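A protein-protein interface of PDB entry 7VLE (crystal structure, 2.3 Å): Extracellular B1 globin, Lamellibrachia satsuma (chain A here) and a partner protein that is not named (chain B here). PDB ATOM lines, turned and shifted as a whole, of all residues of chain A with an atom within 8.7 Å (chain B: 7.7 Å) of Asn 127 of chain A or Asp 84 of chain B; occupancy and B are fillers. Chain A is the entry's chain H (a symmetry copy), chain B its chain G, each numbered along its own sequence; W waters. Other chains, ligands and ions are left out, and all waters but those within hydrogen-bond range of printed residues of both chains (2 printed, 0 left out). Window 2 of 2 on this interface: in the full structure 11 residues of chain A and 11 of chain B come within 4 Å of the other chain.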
ATOM      1  N   ILE A  11      -9.528 -24.253 -10.380  1.00  0.00           N
ATOM      2  CA  ILE A  11      -8.925 -22.931 -10.233  1.00  0.00           C
ATOM      3  C   ILE A  11      -8.964 -22.180 -11.557  1.00  0.00           C
ATOM      4  O   ILE A  11      -9.351 -21.007 -11.615  1.00  0.00           O
ATOM      5  CB  ILE A  11      -7.483 -23.058  -9.707  1.00  0.00           C
ATOM      6  CG1 ILE A  11      -7.466 -23.671  -8.306  1.00  0.00           C
ATOM      7  CG2 ILE A  11      -6.791 -21.706  -9.721  1.00  0.00           C
ATOM      8  CD1 ILE A  11      -6.069 -23.855  -7.746  1.00  0.00           C
ATOM      9  N   GLN A  15     -10.995 -18.702 -12.312  1.00  0.00           N
ATOM     10  CA  GLN A  15     -10.293 -17.468 -12.648  1.00  0.00           C
ATOM     11  C   GLN A  15     -10.660 -16.967 -14.039  1.00  0.00           C
ATOM     12  O   GLN A  15     -10.557 -15.764 -14.310  1.00  0.00           O
ATOM     13  CB  GLN A  15      -8.785 -17.684 -12.536  1.00  0.00           C
ATOM     14  CG  GLN A  15      -8.324 -18.028 -11.129  1.00  0.00           C
ATOM     15  CD  GLN A  15      -6.825 -17.899 -10.950  1.00  0.00           C
ATOM     16  OE1 GLN A  15      -6.063 -17.956 -11.916  1.00  0.00           O
ATOM     17  NE2 GLN A  15      -6.395 -17.715  -9.709  1.00  0.00           N
ATOM     18  N   GLN A  18     -14.089 -15.173 -14.050  1.00  0.00           N
ATOM     19  CA  GLN A  18     -13.917 -13.825 -13.517  1.00  0.00           C
ATOM     20  C   GLN A  18     -13.905 -12.789 -14.635  1.00  0.00           C
ATOM     21  O   GLN A  18     -14.550 -11.700 -14.514  1.00  0.00           O
ATOM     22  CB  GLN A  18     -12.620 -13.811 -12.726  1.00  0.00           C
ATOM     23  CG  GLN A  18     -12.655 -13.070 -11.471  1.00  0.00           C
ATOM     24  CD  GLN A  18     -11.283 -13.085 -10.862  1.00  0.00           C
ATOM     25  OE1 GLN A  18     -10.324 -12.564 -11.447  1.00  0.00           O
ATOM     26  NE2 GLN A  18     -11.162 -13.705  -9.693  1.00  0.00           N
ATOM     27  N   LEU A 121      -3.118 -12.752 -19.308  1.00  0.00           N
ATOM     28  CA  LEU A 121      -4.142 -13.064 -18.312  1.00  0.00           C
ATOM     29  C   LEU A 121      -3.842 -12.560 -16.903  1.00  0.00           C
ATOM     30  O   LEU A 121      -4.782 -12.079 -16.246  1.00  0.00           O
ATOM     31  CB  LEU A 121      -4.387 -14.578 -18.284  1.00  0.00           C
ATOM     32  CG  LEU A 121      -5.111 -15.163 -19.493  1.00  0.00           C
ATOM     33  CD1 LEU A 121      -5.252 -16.668 -19.346  1.00  0.00           C
ATOM     34  CD2 LEU A 121      -6.467 -14.505 -19.657  1.00  0.00           C
ATOM     35  N   PRO A 122      -2.619 -12.658 -16.368  1.00  0.00           N
ATOM     36  CA  PRO A 122      -2.380 -12.107 -15.022  1.00  0.00           C
ATOM     37  C   PRO A 122      -2.675 -10.620 -14.910  1.00  0.00           C
ATOM     38  O   PRO A 122      -2.939 -10.140 -13.801  1.00  0.00           O
ATOM     39  CB  PRO A 122      -0.896 -12.412 -14.765  1.00  0.00           C
ATOM     40  CG  PRO A 122      -0.326 -12.793 -16.092  1.00  0.00           C
ATOM     41  CD  PRO A 122      -1.448 -13.406 -16.854  1.00  0.00           C
ATOM     42  N   SER A 123      -2.644  -9.877 -16.020  1.00  0.00           N
ATOM     43  CA  SER A 123      -3.057  -8.479 -15.990  1.00  0.00           C
ATOM     44  C   SER A 123      -4.557  -8.331 -15.788  1.00  0.00           C
ATOM     45  O   SER A 123      -5.014  -7.258 -15.383  1.00  0.00           O
ATOM     46  CB  SER A 123      -2.645  -7.776 -17.286  1.00  0.00           C
ATOM     47  OG  SER A 123      -1.244  -7.837 -17.482  1.00  0.00           O
ATOM     48  N   LEU A 124      -5.327  -9.388 -16.055  1.00  0.00           N
ATOM     49  CA  LEU A 124      -6.778  -9.338 -15.981  1.00  0.00           C
ATOM     50  C   LEU A 124      -7.364 -10.075 -14.785  1.00  0.00           C
ATOM     51  O   LEU A 124      -8.480  -9.747 -14.373  1.00  0.00           O
ATOM     52  CB  LEU A 124      -7.392  -9.924 -17.263  1.00  0.00           C
ATOM     53  CG  LEU A 124      -7.082  -9.224 -18.587  1.00  0.00           C
ATOM     54  CD1 LEU A 124      -7.674 -10.000 -19.752  1.00  0.00           C
ATOM     55  CD2 LEU A 124      -7.607  -7.798 -18.574  1.00  0.00           C
ATOM     56  N   ILE A 125      -6.648 -11.039 -14.213  1.00  0.00           N
ATOM     57  CA  ILE A 125      -7.221 -11.998 -13.273  1.00  0.00           C
ATOM     58  C   ILE A 125      -6.686 -11.733 -11.871  1.00  0.00           C
ATOM     59  O   ILE A 125      -5.478 -11.544 -11.680  1.00  0.00           O
ATOM     60  CB  ILE A 125      -6.929 -13.442 -13.709  1.00  0.00           C
ATOM     61  CG1 ILE A 125      -7.756 -13.788 -14.948  1.00  0.00           C
ATOM     62  CG2 ILE A 125      -7.213 -14.416 -12.577  1.00  0.00           C
ATOM     63  CD1 ILE A 125      -7.523 -15.184 -15.474  1.00  0.00           C
ATOM     64  N   ASP A 126      -7.593 -11.733 -10.892  1.00  0.00           N
ATOM     65  CA  ASP A 126      -7.217 -11.610  -9.490  1.00  0.00           C
ATOM     66  C   ASP A 126      -6.369 -12.800  -9.057  1.00  0.00           C
ATOM     67  O   ASP A 126      -6.823 -13.947  -9.109  1.00  0.00           O
ATOM     68  CB  ASP A 126      -8.466 -11.514  -8.614  1.00  0.00           C
ATOM     69  CG  ASP A 126      -9.197 -10.197  -8.775  1.00  0.00           C
ATOM     70  OD1 ASP A 126      -8.594  -9.237  -9.303  1.00  0.00           O
ATOM     71  OD2 ASP A 126     -10.372 -10.116  -8.360  1.00  0.00           O
ATOM     72  N   ASN A 127      -5.142 -12.516  -8.624  1.00  0.00           N
ATOM     73  CA  ASN A 127      -4.215 -13.513  -8.090  1.00  0.00           C
ATOM     74  C   ASN A 127      -4.067 -14.704  -9.040  1.00  0.00           C
ATOM     75  O   ASN A 127      -4.310 -15.860  -8.683  1.00  0.00           O
ATOM     76  CB  ASN A 127      -4.647 -13.972  -6.698  1.00  0.00           C
ATOM     77  CG  ASN A 127      -3.491 -14.017  -5.722  1.00  0.00           C
ATOM     78  OD1 ASN A 127      -2.667 -13.103  -5.683  1.00  0.00           O
ATOM     79  ND2 ASN A 127      -3.412 -15.087  -4.944  1.00  0.00           N
ATOM     80  N   PHE A 128      -3.649 -14.390 -10.264  1.00  0.00           N
ATOM     81  CA  PHE A 128      -3.469 -15.389 -11.312  1.00  0.00           C
ATOM     82  C   PHE A 128      -2.544 -16.513 -10.855  1.00  0.00           C
ATOM     83  O   PHE A 128      -1.453 -16.262 -10.338  1.00  0.00           O
ATOM     84  CB  PHE A 128      -2.900 -14.703 -12.556  1.00  0.00           C
ATOM     85  CG  PHE A 128      -2.700 -15.617 -13.730  1.00  0.00           C
ATOM     86  CD1 PHE A 128      -3.777 -16.024 -14.498  1.00  0.00           C
ATOM     87  CD2 PHE A 128      -1.430 -16.044 -14.083  1.00  0.00           C
ATOM     88  CE1 PHE A 128      -3.594 -16.856 -15.587  1.00  0.00           C
ATOM     89  CE2 PHE A 128      -1.240 -16.876 -15.170  1.00  0.00           C
ATOM     90  CZ  PHE A 128      -2.324 -17.282 -15.924  1.00  0.00           C
ATOM     91  N   ASN A 129      -2.993 -17.761 -11.048  1.00  0.00           N
ATOM     92  CA  ASN A 129      -2.206 -18.934 -10.686  1.00  0.00           C
ATOM     93  C   ASN A 129      -1.518 -19.480 -11.931  1.00  0.00           C
ATOM     94  O   ASN A 129      -2.131 -20.251 -12.687  1.00  0.00           O
ATOM     95  CB  ASN A 129      -3.083 -20.011 -10.037  1.00  0.00           C
ATOM     96  CG  ASN A 129      -2.267 -21.171  -9.461  1.00  0.00           C
ATOM     97  OD1 ASN A 129      -1.218 -21.537  -9.989  1.00  0.00           O
ATOM     98  ND2 ASN A 129      -2.760 -21.753  -8.373  1.00  0.00           N
ATOM     99  N   PRO A 130      -0.250 -19.144 -12.169  1.00  0.00           N
ATOM    100  CA  PRO A 130       0.425 -19.590 -13.397  1.00  0.00           C
ATOM    101  C   PRO A 130       0.729 -21.076 -13.424  1.00  0.00           C
ATOM    102  O   PRO A 130       1.020 -21.608 -14.501  1.00  0.00           O
ATOM    103  CB  PRO A 130       1.718 -18.769 -13.394  1.00  0.00           C
ATOM    104  CG  PRO A 130       1.993 -18.549 -11.932  1.00  0.00           C
ATOM    105  CD  PRO A 130       0.648 -18.385 -11.281  1.00  0.00           C
ATOM    106  N   ASP A 131       0.688 -21.756 -12.277  1.00  0.00           N
ATOM    107  CA  ASP A 131       0.988 -23.183 -12.243  1.00  0.00           C
ATOM    108  C   ASP A 131      -0.201 -24.012 -12.711  1.00  0.00           C
ATOM    109  O   ASP A 131      -0.056 -24.886 -13.574  1.00  0.00           O
ATOM    110  CB  ASP A 131       1.404 -23.603 -10.833  1.00  0.00           C
ATOM    111  CG  ASP A 131       2.886 -23.432 -10.587  1.00  0.00           C
ATOM    112  OD1 ASP A 131       3.396 -24.021  -9.610  1.00  0.00           O
ATOM    113  OD2 ASP A 131       3.541 -22.705 -11.363  1.00  0.00           O
ATOM    114  N   TRP A 133      -2.798 -22.954 -14.422  1.00  0.00           N
ATOM    115  CA  TRP A 133      -3.072 -22.607 -15.813  1.00  0.00           C
ATOM    116  C   TRP A 133      -2.115 -23.323 -16.756  1.00  0.00           C
ATOM    117  O   TRP A 133      -2.531 -23.870 -17.785  1.00  0.00           O
ATOM    118  CB  TRP A 133      -2.980 -21.092 -16.000  1.00  0.00           C
ATOM    119  CG  TRP A 133      -4.230 -20.365 -15.618  1.00  0.00           C
ATOM    120  CD1 TRP A 133      -4.565 -19.898 -14.382  1.00  0.00           C
ATOM    121  CD2 TRP A 133      -5.317 -20.023 -16.485  1.00  0.00           C
ATOM    122  NE1 TRP A 133      -5.794 -19.284 -14.424  1.00  0.00           N
ATOM    123  CE2 TRP A 133      -6.276 -19.348 -15.706  1.00  0.00           C
ATOM    124  CE3 TRP A 133      -5.570 -20.222 -17.846  1.00  0.00           C
ATOM    125  CZ2 TRP A 133      -7.471 -18.871 -16.240  1.00  0.00           C
ATOM    126  CZ3 TRP A 133      -6.758 -19.748 -18.375  1.00  0.00           C
ATOM    127  CH2 TRP A 133      -7.691 -19.080 -17.574  1.00  0.00           C
ATOM    128  N   ARG B  10       0.070 -30.300  -3.905  1.00  0.00           N
ATOM    129  CA  ARG B  10       0.611 -29.231  -3.072  1.00  0.00           C
ATOM    130  C   ARG B  10       0.038 -29.285  -1.661  1.00  0.00           C
ATOM    131  O   ARG B  10       0.783 -29.229  -0.676  1.00  0.00           O
ATOM    132  CB  ARG B  10       0.329 -27.875  -3.720  1.00  0.00           C
ATOM    133  CG  ARG B  10       1.217 -27.578  -4.909  1.00  0.00           C
ATOM    134  CD  ARG B  10       0.490 -26.810  -6.002  1.00  0.00           C
ATOM    135  NE  ARG B  10       1.106 -27.030  -7.309  1.00  0.00           N
ATOM    136  CZ  ARG B  10       1.916 -26.168  -7.915  1.00  0.00           C
ATOM    137  NH1 ARG B  10       2.206 -25.009  -7.340  1.00  0.00           N
ATOM    138  NH2 ARG B  10       2.431 -26.462  -9.102  1.00  0.00           N
ATOM    139  N   GLN B  14       2.142 -29.951   1.749  1.00  0.00           N
ATOM    140  CA  GLN B  14       2.096 -29.017   2.867  1.00  0.00           C
ATOM    141  C   GLN B  14       1.716 -29.720   4.163  1.00  0.00           C
ATOM    142  O   GLN B  14       2.189 -29.331   5.237  1.00  0.00           O
ATOM    143  CB  GLN B  14       1.127 -27.875   2.549  1.00  0.00           C
ATOM    144  CG  GLN B  14       1.718 -26.832   1.603  1.00  0.00           C
ATOM    145  CD  GLN B  14       0.683 -25.884   1.022  1.00  0.00           C
ATOM    146  OE1 GLN B  14      -0.521 -26.080   1.185  1.00  0.00           O
ATOM    147  NE2 GLN B  14       1.153 -24.849   0.335  1.00  0.00           N
ATOM    148  N   ALA B  78       9.391 -22.177   0.356  1.00  0.00           N
ATOM    149  CA  ALA B  78       8.990 -22.651  -0.963  1.00  0.00           C
ATOM    150  C   ALA B  78       7.731 -23.505  -0.879  1.00  0.00           C
ATOM    151  O   ALA B  78       6.797 -23.330  -1.671  1.00  0.00           O
ATOM    152  CB  ALA B  78      10.135 -23.436  -1.601  1.00  0.00           C
ATOM    153  N   ILE B  79       7.692 -24.441   0.073  1.00  0.00           N
ATOM    154  CA  ILE B  79       6.514 -25.287   0.248  1.00  0.00           C
ATOM    155  C   ILE B  79       5.293 -24.440   0.577  1.00  0.00           C
ATOM    156  O   ILE B  79       4.182 -24.712   0.104  1.00  0.00           O
ATOM    157  CB  ILE B  79       6.775 -26.346   1.337  1.00  0.00           C
ATOM    158  CG1 ILE B  79       7.828 -27.353   0.874  1.00  0.00           C
ATOM    159  CG2 ILE B  79       5.485 -27.059   1.718  1.00  0.00           C
ATOM    160  CD1 ILE B  79       8.070 -28.470   1.865  1.00  0.00           C
ATOM    161  N   GLY B  80       5.478 -23.400   1.391  1.00  0.00           N
ATOM    162  CA  GLY B  80       4.362 -22.543   1.747  1.00  0.00           C
ATOM    163  C   GLY B  80       3.869 -21.696   0.594  1.00  0.00           C
ATOM    164  O   GLY B  80       2.680 -21.375   0.520  1.00  0.00           O
ATOM    165  N   LEU B  81       4.763 -21.321  -0.318  1.00  0.00           N
ATOM    166  CA  LEU B  81       4.395 -20.514  -1.472  1.00  0.00           C
ATOM    167  C   LEU B  81       3.869 -21.346  -2.632  1.00  0.00           C
ATOM    168  O   LEU B  81       3.519 -20.779  -3.672  1.00  0.00           O
ATOM    169  CB  LEU B  81       5.587 -19.669  -1.926  1.00  0.00           C
ATOM    170  CG  LEU B  81       5.878 -18.488  -0.997  1.00  0.00           C
ATOM    171  CD1 LEU B  81       7.125 -17.739  -1.435  1.00  0.00           C
ATOM    172  CD2 LEU B  81       4.674 -17.559  -0.936  1.00  0.00           C
ATOM    173  N   LEU B  82       3.804 -22.673  -2.478  1.00  0.00           N
ATOM    174  CA  LEU B  82       3.106 -23.508  -3.448  1.00  0.00           C
ATOM    175  C   LEU B  82       1.653 -23.088  -3.612  1.00  0.00           C
ATOM    176  O   LEU B  82       1.052 -23.359  -4.657  1.00  0.00           O
ATOM    177  CB  LEU B  82       3.172 -24.977  -3.025  1.00  0.00           C
ATOM    178  CG  LEU B  82       4.518 -25.691  -3.153  1.00  0.00           C
ATOM    179  CD1 LEU B  82       4.441 -27.091  -2.561  1.00  0.00           C
ATOM    180  CD2 LEU B  82       4.946 -25.748  -4.608  1.00  0.00           C
ATOM    181  N   SER B  83       1.080 -22.440  -2.598  1.00  0.00           N
ATOM    182  CA  SER B  83      -0.274 -21.912  -2.659  1.00  0.00           C
ATOM    183  C   SER B  83      -0.367 -20.609  -3.442  1.00  0.00           C
ATOM    184  O   SER B  83      -1.481 -20.168  -3.745  1.00  0.00           O
ATOM    185  CB  SER B  83      -0.809 -21.696  -1.241  1.00  0.00           C
ATOM    186  OG  SER B  83      -0.777 -22.903  -0.499  1.00  0.00           O
ATOM    187  N   ASP B  84       0.762 -19.984  -3.767  1.00  0.00           N
ATOM    188  CA  ASP B  84       0.783 -18.735  -4.531  1.00  0.00           C
ATOM    189  C   ASP B  84       1.970 -18.767  -5.481  1.00  0.00           C
ATOM    190  O   ASP B  84       3.016 -18.158  -5.225  1.00  0.00           O
ATOM    191  CB  ASP B  84       0.845 -17.521  -3.604  1.00  0.00           C
ATOM    192  CG  ASP B  84       0.775 -16.214  -4.361  1.00  0.00           C
ATOM    193  OD1 ASP B  84       0.172 -16.190  -5.454  1.00  0.00           O
ATOM    194  OD2 ASP B  84       1.341 -15.217  -3.869  1.00  0.00           O
ATOM    195  N   PRO B  85       1.831 -19.465  -6.611  1.00  0.00           N
ATOM    196  CA  PRO B  85       2.979 -19.679  -7.509  1.00  0.00           C
ATOM    197  C   PRO B  85       3.597 -18.402  -8.051  1.00  0.00           C
ATOM    198  O   PRO B  85       4.805 -18.383  -8.324  1.00  0.00           O
ATOM    199  CB  PRO B  85       2.377 -20.529  -8.636  1.00  0.00           C
ATOM    200  CG  PRO B  85       1.189 -21.194  -8.010  1.00  0.00           C
ATOM    201  CD  PRO B  85       0.631 -20.193  -7.054  1.00  0.00           C
ATOM    202  N   SER B  86       2.802 -17.344  -8.234  1.00  0.00           N
ATOM    203  CA  SER B  86       3.344 -16.062  -8.676  1.00  0.00           C
ATOM    204  C   SER B  86       4.462 -15.594  -7.754  1.00  0.00           C
ATOM    205  O   SER B  86       5.560 -15.250  -8.205  1.00  0.00           O
ATOM    206  CB  SER B  86       2.231 -15.015  -8.731  1.00  0.00           C
ATOM    207  OG  SER B  86       1.193 -15.404  -9.612  1.00  0.00           O
ATOM    208  N   THR B  87       4.187 -15.573  -6.448  1.00  0.00           N
ATOM    209  CA  THR B  87       5.208 -15.213  -5.470  1.00  0.00           C
ATOM    210  C   THR B  87       6.291 -16.280  -5.391  1.00  0.00           C
ATOM    211  O   THR B  87       7.473 -15.964  -5.209  1.00  0.00           O
ATOM    212  CB  THR B  87       4.558 -15.007  -4.101  1.00  0.00           C
ATOM    213  OG1 THR B  87       3.491 -14.056  -4.215  1.00  0.00           O
ATOM    214  CG2 THR B  87       5.574 -14.506  -3.086  1.00  0.00           C
ATOM    215  N   LEU B  88       5.900 -17.550  -5.529  1.00  0.00           N
ATOM    216  CA  LEU B  88       6.856 -18.653  -5.481  1.00  0.00           C
ATOM    217  C   LEU B  88       7.941 -18.489  -6.536  1.00  0.00           C
ATOM    218  O   LEU B  88       9.135 -18.631  -6.244  1.00  0.00           O
ATOM    219  CB  LEU B  88       6.124 -19.980  -5.676  1.00  0.00           C
ATOM    220  CG  LEU B  88       7.012 -21.209  -5.876  1.00  0.00           C
ATOM    221  CD1 LEU B  88       7.681 -21.600  -4.567  1.00  0.00           C
ATOM    222  CD2 LEU B  88       6.215 -22.369  -6.454  1.00  0.00           C
ATOM    223  N   ASN B  89       7.539 -18.201  -7.779  1.00  0.00           N
ATOM    224  CA  ASN B  89       8.504 -17.995  -8.855  1.00  0.00           C
ATOM    225  C   ASN B  89       9.541 -16.945  -8.476  1.00  0.00           C
ATOM    226  O   ASN B  89      10.727 -17.090  -8.790  1.00  0.00           O
ATOM    227  CB  ASN B  89       7.775 -17.589 -10.139  1.00  0.00           C
ATOM    228  CG  ASN B  89       6.993 -18.732 -10.759  1.00  0.00           C
ATOM    229  OD1 ASN B  89       7.371 -19.897 -10.635  1.00  0.00           O
ATOM    230  ND2 ASN B  89       5.899 -18.404 -11.439  1.00  0.00           N
ATOM    231  N   GLU B  90       9.107 -15.887  -7.786  1.00  0.00           N
ATOM    232  CA  GLU B  90      10.029 -14.842  -7.349  1.00  0.00           C
ATOM    233  C   GLU B  90      10.987 -15.350  -6.279  1.00  0.00           C
ATOM    234  O   GLU B  90      12.182 -15.037  -6.310  1.00  0.00           O
ATOM    235  CB  GLU B  90       9.245 -13.639  -6.829  1.00  0.00           C
ATOM    236  CG  GLU B  90       8.595 -12.824  -7.917  1.00  0.00           C
ATOM    237  CD  GLU B  90       9.590 -12.409  -8.978  1.00  0.00           C
ATOM    238  OE1 GLU B  90      10.526 -11.648  -8.653  1.00  0.00           O
ATOM    239  OE2 GLU B  90       9.448 -12.863 -10.132  1.00  0.00           O
ATOM    240  N   ARG B 139       9.376 -29.641  -8.830  1.00  0.00           N
ATOM    241  CA  ARG B 139       8.880 -28.336  -9.252  1.00  0.00           C
ATOM    242  C   ARG B 139       9.628 -27.211  -8.552  1.00  0.00           C
ATOM    243  O   ARG B 139       9.881 -26.161  -9.154  1.00  0.00           O
ATOM    244  CB  ARG B 139       7.375 -28.247  -8.969  1.00  0.00           C
ATOM    245  CG  ARG B 139       6.810 -26.836  -8.878  1.00  0.00           C
ATOM    246  CD  ARG B 139       6.768 -26.156 -10.234  1.00  0.00           C
ATOM    247  NE  ARG B 139       6.170 -24.825 -10.160  1.00  0.00           N
ATOM    248  CZ  ARG B 139       6.862 -23.701 -10.003  1.00  0.00           C
ATOM    249  NH1 ARG B 139       8.184 -23.744  -9.906  1.00  0.00           N
ATOM    250  NH2 ARG B 139       6.234 -22.535  -9.947  1.00  0.00           N
HETATM  251  O   HOH W   1       4.482 -20.942 -12.900  1.00  0.00           O
HETATM  252  O   HOH W   2      -0.854 -17.024  -7.918  1.00  0.00           O
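OD1 of Asp 131 of chain A lies within salt-bridge range of NE of Arg 139 of chain B (2.9 Å). The guanidinium group (NH2) of Arg 10 of chain B is in salt-bridge range of the side-chain carboxylate (OD1) of Asp 131 of chain A. OG of Ser 86 of chain B lies within hydrogen-bond range of O of Phe 128 of chain A (2.9 Å).
The backbone carbonyl oxygen (O) of Asn 127 of chain A lies within hydrogen-bond range of the side-chain amide nitrogen (NE2) of Gln 15 of chain A (3.0 Å). N of Asn 129 of chain A is in hydrogen-bond range of OE1 of Gln 15 of chain A (3.2 Å). NH1 of Arg 10 of chain B is in hydrogen-bond range of O of Leu 82 of chain B (3.4 Å). The backbone carbonyl oxygen (O) of Pro 85 of chain B sits close to the side-chain amide nitrogen (ND2) of Asn 89 of chain B (3.3 Å). The side-chain carboxylate (OD2) of Asp 84 of chain B lies within hydrogen-bond range of the side-chain hydroxyl (OG1) of Thr 87 of chain B (2.5 Å). The guanidinium group (NH2) of Arg 139 of chain B is in hydrogen-bond range of the side-chain amide oxygen (OD1) of Asn 89 of chain B, 3.0 Å away.
Asn 127 of chain A touches Asp 84 of chain B (ND2 to OD1, 3.8 Å). Asn 129 of chain A touches Pro 85 of chain B. Pro 130 of chain A touches Pro 85 of chain B. Ser 86 of chain B touches Pro 130 of chain A (OG to CD, 3.5 Å). CG of Pro 130 of chain A touches ND2 of Asn 89 of chain B (3.9 Å). Asp 131 of chain A touches Pro 85 of chain B.
Of the printed residues of chain B, Asn 127 of chain A touches Asp 84 (3.8 Å). Asp 84 of chain B touches just one residue of chain A: Asn 127 (3.8 Å). Ser 83 of chain B touches none of the printed residues of chain A. Of chain A, only Asn 129 (3.1 Å), Pro 130 (3.8 Å) and Asp 131 (3.5 Å) come within 4 Å of Pro 85 of chain B. Of the printed residues of chain A, Asn 89 of chain B touches Pro 130 (3.9 Å). Of the printed residues of chain A, Arg 10 of chain B touches Asp 131. Of the printed residues of chain B, Phe 128 of chain A touches Ser 86 (2.9 Å). Of the printed residues of chain B, Asp 131 of chain A touches Arg 10 (2.7 Å), Pro 85 (3.5 Å) and Arg 139 (2.9 Å). The nearest residue of chain A that does not touch Asp 84 of chain B is Phe 128 of chain A (5.1 Å). The nearest printed residue of chain B that does not touch Phe 128 of chain A is Asp 84 of chain B (5.1 Å).
Of the 16 printed residues of chain B, 6 touch a printed residue of chain A. Printed residues of chain B that touch a printed residue of chain A: Arg 10, Asp 84, Pro 85, Ser 86, Asn 89 and Arg 139. Hydrophobic or aromatic side chains of chain B that line the printed part of chain A: Pro 85. Of the 15 printed residues of chain A, 5 touch a printed residue of chain B.
Water W1 bridges OD2 of Asp 131 of chain A (2.5 Å) and ND2 of Asn 89 of chain B (3.3 Å). Water W2 lies within hydrogen-bond range of the backbone carbonyl oxygen (O) of Phe 128 of chain A (2.6 Å), the side-chain carboxylate (OD1) of Asp 84 of chain B (2.8 Å) and the side-chain hydroxyl (OG) of Ser 86 of chain B (3.1 Å).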
